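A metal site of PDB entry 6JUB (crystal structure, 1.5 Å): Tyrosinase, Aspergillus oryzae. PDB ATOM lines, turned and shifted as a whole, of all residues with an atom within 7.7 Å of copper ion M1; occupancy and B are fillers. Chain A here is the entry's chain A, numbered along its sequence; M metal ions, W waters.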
ATOM      1  N   HIS A  71       3.418 -11.751  -9.594  1.00  0.00           N
ATOM      2  CA  HIS A  71       4.775 -11.261  -9.649  1.00  0.00           C
ATOM      3  C   HIS A  71       4.917  -9.896  -8.997  1.00  0.00           C
ATOM      4  O   HIS A  71       5.910  -9.655  -8.308  1.00  0.00           O
ATOM      5  CB  HIS A  71       5.257 -11.231 -11.104  1.00  0.00           C
ATOM      6  CG  HIS A  71       6.718 -10.947 -11.293  1.00  0.00           C
ATOM      7  ND1 HIS A  71       7.200  -9.734 -11.735  1.00  0.00           N
ATOM      8  CD2 HIS A  71       7.820 -11.726 -11.100  1.00  0.00           C
ATOM      9  CE1 HIS A  71       8.522  -9.778 -11.808  1.00  0.00           C
ATOM     10  NE2 HIS A  71       8.927 -10.982 -11.423  1.00  0.00           N
ATOM     11  N   VAL A  97      10.664 -12.959  -5.867  1.00  0.00           N
ATOM     12  CA  VAL A  97      11.952 -12.769  -5.213  1.00  0.00           C
ATOM     13  C   VAL A  97      12.974 -12.205  -6.207  1.00  0.00           C
ATOM     14  O   VAL A  97      13.259 -12.826  -7.231  1.00  0.00           O
ATOM     15  CB  VAL A  97      12.538 -14.066  -4.632  1.00  0.00           C
ATOM     16  CG1 VAL A  97      13.930 -13.792  -4.089  1.00  0.00           C
ATOM     17  CG2 VAL A  97      11.633 -14.623  -3.546  1.00  0.00           C
ATOM     18  N   HIS A  98      13.519 -11.050  -5.851  1.00  0.00           N
ATOM     19  CA  HIS A  98      14.598 -10.441  -6.625  1.00  0.00           C
ATOM     20  C   HIS A  98      15.725 -10.043  -5.684  1.00  0.00           C
ATOM     21  O   HIS A  98      15.463  -9.755  -4.513  1.00  0.00           O
ATOM     22  CB  HIS A  98      14.100  -9.229  -7.428  1.00  0.00           C
ATOM     23  CG  HIS A  98      12.975  -9.581  -8.365  1.00  0.00           C
ATOM     24  ND1 HIS A  98      11.702  -9.070  -8.239  1.00  0.00           N
ATOM     25  CD2 HIS A  98      12.935 -10.412  -9.432  1.00  0.00           C
ATOM     26  CE1 HIS A  98      10.934  -9.571  -9.190  1.00  0.00           C
ATOM     27  NE2 HIS A  98      11.649 -10.392  -9.936  1.00  0.00           N
ATOM     28  N   PHE A 103      16.162 -16.284  -5.998  1.00  0.00           N
ATOM     29  CA  PHE A 103      15.651 -15.793  -7.283  1.00  0.00           C
ATOM     30  C   PHE A 103      15.431 -16.918  -8.283  1.00  0.00           C
ATOM     31  O   PHE A 103      14.336 -16.966  -8.886  1.00  0.00           O
ATOM     32  CB  PHE A 103      16.587 -14.707  -7.838  1.00  0.00           C
ATOM     33  CG  PHE A 103      16.426 -14.470  -9.321  1.00  0.00           C
ATOM     34  CD1 PHE A 103      15.406 -13.683  -9.838  1.00  0.00           C
ATOM     35  CD2 PHE A 103      17.307 -15.033 -10.226  1.00  0.00           C
ATOM     36  CE1 PHE A 103      15.265 -13.492 -11.197  1.00  0.00           C
ATOM     37  CE2 PHE A 103      17.185 -14.842 -11.597  1.00  0.00           C
ATOM     38  CZ  PHE A 103      16.164 -14.048 -12.091  1.00  0.00           C
ATOM     39  N   HIS A 107      11.413 -18.401  -9.203  1.00  0.00           N
ATOM     40  CA  HIS A 107      10.907 -18.309 -10.583  1.00  0.00           C
ATOM     41  C   HIS A 107      10.768 -19.686 -11.223  1.00  0.00           C
ATOM     42  O   HIS A 107       9.940 -19.853 -12.119  1.00  0.00           O
ATOM     43  CB  HIS A 107      11.793 -17.396 -11.441  1.00  0.00           C
ATOM     44  CG  HIS A 107      11.663 -15.950 -11.045  1.00  0.00           C
ATOM     45  ND1 HIS A 107      12.362 -15.397 -10.009  1.00  0.00           N
ATOM     46  CD2 HIS A 107      10.919 -14.956 -11.571  1.00  0.00           C
ATOM     47  CE1 HIS A 107      12.044 -14.117  -9.890  1.00  0.00           C
ATOM     48  NE2 HIS A 107      11.160 -13.829 -10.833  1.00  0.00           N
ATOM     49  N   GLU A 329      21.099 -13.487 -12.421  1.00  0.00           N
ATOM     50  CA  GLU A 329      20.089 -12.453 -12.277  1.00  0.00           C
ATOM     51  C   GLU A 329      20.469 -11.207 -13.051  1.00  0.00           C
ATOM     52  O   GLU A 329      19.600 -10.565 -13.657  1.00  0.00           O
ATOM     53  CB  GLU A 329      19.854 -12.163 -10.792  1.00  0.00           C
ATOM     54  CG  GLU A 329      18.593 -11.314 -10.562  1.00  0.00           C
ATOM     55  CD  GLU A 329      18.290 -11.111  -9.095  1.00  0.00           C
ATOM     56  OE1 GLU A 329      19.075 -11.525  -8.228  1.00  0.00           O
ATOM     57  OE2 GLU A 329      17.229 -10.514  -8.804  1.00  0.00           O
ATOM     58  N   HIS A 332      19.713 -11.661 -16.695  1.00  0.00           N
ATOM     59  CA  HIS A 332      18.255 -11.618 -16.798  1.00  0.00           C
ATOM     60  C   HIS A 332      17.728 -10.195 -16.732  1.00  0.00           C
ATOM     61  O   HIS A 332      16.754  -9.841 -17.414  1.00  0.00           O
ATOM     62  CB  HIS A 332      17.635 -12.508 -15.718  1.00  0.00           C
ATOM     63  CG  HIS A 332      16.416 -12.005 -15.032  1.00  0.00           C
ATOM     64  ND1 HIS A 332      16.430 -11.022 -14.062  1.00  0.00           N
ATOM     65  CD2 HIS A 332      15.121 -12.379 -15.137  1.00  0.00           C
ATOM     66  CE1 HIS A 332      15.192 -10.811 -13.624  1.00  0.00           C
ATOM     67  NE2 HIS A 332      14.369 -11.622 -14.265  1.00  0.00           N
ATOM     68  N   ASN A 333      18.381  -9.360 -15.941  1.00  0.00           N
ATOM     69  CA  ASN A 333      17.940  -7.968 -15.782  1.00  0.00           C
ATOM     70  C   ASN A 333      18.173  -7.208 -17.079  1.00  0.00           C
ATOM     71  O   ASN A 333      17.337  -6.433 -17.521  1.00  0.00           O
ATOM     72  CB  ASN A 333      18.710  -7.273 -14.655  1.00  0.00           C
ATOM     73  CG  ASN A 333      18.331  -7.693 -13.263  1.00  0.00           C
ATOM     74  OD1 ASN A 333      17.336  -8.397 -13.039  1.00  0.00           O
ATOM     75  ND2 ASN A 333      19.145  -7.276 -12.283  1.00  0.00           N
ATOM     76  N   HIS A 336      15.501  -8.098 -19.638  1.00  0.00           N
ATOM     77  CA  HIS A 336      14.269  -7.356 -19.366  1.00  0.00           C
ATOM     78  C   HIS A 336      14.268  -5.962 -20.003  1.00  0.00           C
ATOM     79  O   HIS A 336      13.318  -5.564 -20.670  1.00  0.00           O
ATOM     80  CB  HIS A 336      14.073  -7.245 -17.847  1.00  0.00           C
ATOM     81  CG  HIS A 336      13.257  -8.310 -17.202  1.00  0.00           C
ATOM     82  ND1 HIS A 336      11.882  -8.394 -17.317  1.00  0.00           N
ATOM     83  CD2 HIS A 336      13.599  -9.349 -16.407  1.00  0.00           C
ATOM     84  CE1 HIS A 336      11.433  -9.432 -16.633  1.00  0.00           C
ATOM     85  NE2 HIS A 336      12.450 -10.026 -16.066  1.00  0.00           N
ATOM     86  N   MET A 360       8.240  -4.976 -20.087  1.00  0.00           N
ATOM     87  CA  MET A 360       9.256  -5.929 -19.665  1.00  0.00           C
ATOM     88  C   MET A 360      10.398  -5.266 -18.897  1.00  0.00           C
ATOM     89  O   MET A 360      11.134  -5.968 -18.200  1.00  0.00           O
ATOM     90  CB  MET A 360       9.794  -6.710 -20.862  1.00  0.00           C
ATOM     91  CG  MET A 360       9.055  -7.991 -21.176  1.00  0.00           C
ATOM     92  SD  MET A 360       9.309  -9.301 -19.948  1.00  0.00           S
ATOM     93  CE  MET A 360      10.903  -9.902 -20.440  1.00  0.00           C
ATOM     94  N   VAL A 363       9.703  -4.080 -13.111  1.00  0.00           N
ATOM     95  CA  VAL A 363       9.351  -5.168 -12.197  1.00  0.00           C
ATOM     96  C   VAL A 363       7.868  -5.300 -11.906  1.00  0.00           C
ATOM     97  O   VAL A 363       7.330  -6.416 -11.963  1.00  0.00           O
ATOM     98  CB  VAL A 363      10.121  -5.018 -10.871  1.00  0.00           C
ATOM     99  CG1 VAL A 363       9.632  -6.083  -9.897  1.00  0.00           C
ATOM    100  CG2 VAL A 363      11.618  -5.127 -11.104  1.00  0.00           C
ATOM    101  N   ALA A 366       6.150  -6.393 -15.533  1.00  0.00           N
ATOM    102  CA  ALA A 366       6.816  -7.187 -16.560  1.00  0.00           C
ATOM    103  C   ALA A 366       6.090  -8.504 -16.829  1.00  0.00           C
ATOM    104  O   ALA A 366       6.078  -8.953 -17.987  1.00  0.00           O
ATOM    105  CB  ALA A 366       8.276  -7.455 -16.205  1.00  0.00           C
ATOM    106  N   ALA A 367       5.503  -9.127 -15.815  1.00  0.00           N
ATOM    107  CA  ALA A 367       4.899 -10.453 -16.017  1.00  0.00           C
ATOM    108  C   ALA A 367       3.686 -10.412 -16.925  1.00  0.00           C
ATOM    109  O   ALA A 367       3.268 -11.452 -17.446  1.00  0.00           O
ATOM    110  CB  ALA A 367       4.541 -11.059 -14.662  1.00  0.00           C
ATOM    111  N   PHE A 372       7.561 -12.626 -21.033  1.00  0.00           N
ATOM    112  CA  PHE A 372       8.130 -12.781 -19.697  1.00  0.00           C
ATOM    113  C   PHE A 372       8.359 -14.247 -19.346  1.00  0.00           C
ATOM    114  O   PHE A 372       9.400 -14.642 -18.820  1.00  0.00           O
ATOM    115  CB  PHE A 372       7.162 -12.157 -18.685  1.00  0.00           C
ATOM    116  CG  PHE A 372       7.535 -12.425 -17.260  1.00  0.00           C
ATOM    117  CD1 PHE A 372       7.082 -13.560 -16.608  1.00  0.00           C
ATOM    118  CD2 PHE A 372       8.337 -11.534 -16.557  1.00  0.00           C
ATOM    119  CE1 PHE A 372       7.428 -13.802 -15.276  1.00  0.00           C
ATOM    120  CE2 PHE A 372       8.686 -11.772 -15.239  1.00  0.00           C
ATOM    121  CZ  PHE A 372       8.228 -12.899 -14.586  1.00  0.00           C
ATOM    122  N   HIS A 375      11.152 -15.914 -21.401  1.00  0.00           N
ATOM    123  CA  HIS A 375      12.421 -15.451 -20.864  1.00  0.00           C
ATOM    124  C   HIS A 375      12.747 -16.192 -19.575  1.00  0.00           C
ATOM    125  O   HIS A 375      13.839 -16.741 -19.369  1.00  0.00           O
ATOM    126  CB  HIS A 375      12.317 -13.943 -20.611  1.00  0.00           C
ATOM    127  CG  HIS A 375      13.463 -13.315 -19.888  1.00  0.00           C
ATOM    128  ND1 HIS A 375      14.765 -13.619 -20.200  1.00  0.00           N
ATOM    129  CD2 HIS A 375      13.533 -12.389 -18.887  1.00  0.00           C
ATOM    130  CE1 HIS A 375      15.584 -12.914 -19.425  1.00  0.00           C
ATOM    131  NE2 HIS A 375      14.865 -12.164 -18.609  1.00  0.00           N
ATOM    132  N   HIS A 376      11.766 -16.279 -18.667  1.00  0.00           N
ATOM    133  CA  HIS A 376      11.999 -17.004 -17.417  1.00  0.00           C
ATOM    134  C   HIS A 376      12.133 -18.499 -17.656  1.00  0.00           C
ATOM    135  O   HIS A 376      12.799 -19.175 -16.860  1.00  0.00           O
ATOM    136  CB  HIS A 376      10.934 -16.674 -16.355  1.00  0.00           C
ATOM    137  CG  HIS A 376      11.456 -15.481 -15.587  1.00  0.00           C
ATOM    138  ND1 HIS A 376      12.440 -15.577 -14.624  1.00  0.00           N
ATOM    139  CD2 HIS A 376      11.164 -14.176 -15.723  1.00  0.00           C
ATOM    140  CE1 HIS A 376      12.701 -14.368 -14.157  1.00  0.00           C
ATOM    141  NE2 HIS A 376      11.938 -13.507 -14.809  1.00  0.00           N
ATOM    142  N   ILE A 379      15.685 -18.668 -18.299  1.00  0.00           N
ATOM    143  CA  ILE A 379      16.442 -18.476 -17.052  1.00  0.00           C
ATOM    144  C   ILE A 379      16.457 -19.770 -16.246  1.00  0.00           C
ATOM    145  O   ILE A 379      17.494 -20.155 -15.660  1.00  0.00           O
ATOM    146  CB  ILE A 379      15.903 -17.268 -16.276  1.00  0.00           C
ATOM    147  CG1 ILE A 379      16.106 -15.962 -17.054  1.00  0.00           C
ATOM    148  CG2 ILE A 379      16.479 -17.137 -14.873  1.00  0.00           C
ATOM    149  CD1 ILE A 379      17.569 -15.650 -17.331  1.00  0.00           C
ATOM    150  N   PHE A 517      17.044  -3.540 -12.617  1.00  0.00           N
ATOM    151  CA  PHE A 517      15.663  -4.007 -12.692  1.00  0.00           C
ATOM    152  C   PHE A 517      15.032  -3.896 -11.304  1.00  0.00           C
ATOM    153  O   PHE A 517      15.129  -4.813 -10.478  1.00  0.00           O
ATOM    154  CB  PHE A 517      15.639  -5.445 -13.183  1.00  0.00           C
ATOM    155  CG  PHE A 517      14.295  -6.039 -13.513  1.00  0.00           C
ATOM    156  CD1 PHE A 517      13.434  -5.453 -14.413  1.00  0.00           C
ATOM    157  CD2 PHE A 517      13.925  -7.227 -12.907  1.00  0.00           C
ATOM    158  CE1 PHE A 517      12.223  -6.045 -14.709  1.00  0.00           C
ATOM    159  CE2 PHE A 517      12.714  -7.818 -13.203  1.00  0.00           C
ATOM    160  CZ  PHE A 517      11.859  -7.238 -14.118  1.00  0.00           C
HETATM  161 CU    CU M   1      12.452 -11.487 -14.627  1.00  0.00          CU
HETATM  162 CU    CU M   2      10.741 -11.746 -11.297  1.00  0.00          CU
HETATM  163  O   HOH W   1      11.248 -11.063 -13.347  1.00  0.00           O
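O of His 332 sits at hydrogen-bond distance from NE2 of His 375.
The side-chain amide oxygen (OD1) of Asn 333 sits at hydrogen-bond distance from a ring nitrogen (ND1) of His 332, at 3.0 Å.
A ring nitrogen (ND1) of His 332 lies within hydrogen-bond range of the backbone carbonyl oxygen of Glu 329.
A ring nitrogen (ND1) of His 336 lies within hydrogen-bond range of the backbone carbonyl oxygen (O) of Met 360 (2.7 Å).
Phe 372 touches copper ion M1 (CE2 to CU, 3.8 Å).
Phe 517 touches copper ion M1.
Five residues have an atom within 4 Å of copper ion M1: His 332, His 336, Phe 372, His 376 and Phe 517.
Copper ion M1 is bound by water W1 (1.8 Å), NE2 of His 332 (2.0 Å), NE2 of His 336 (2.1 Å) and NE2 of His 376 (2.1 Å).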
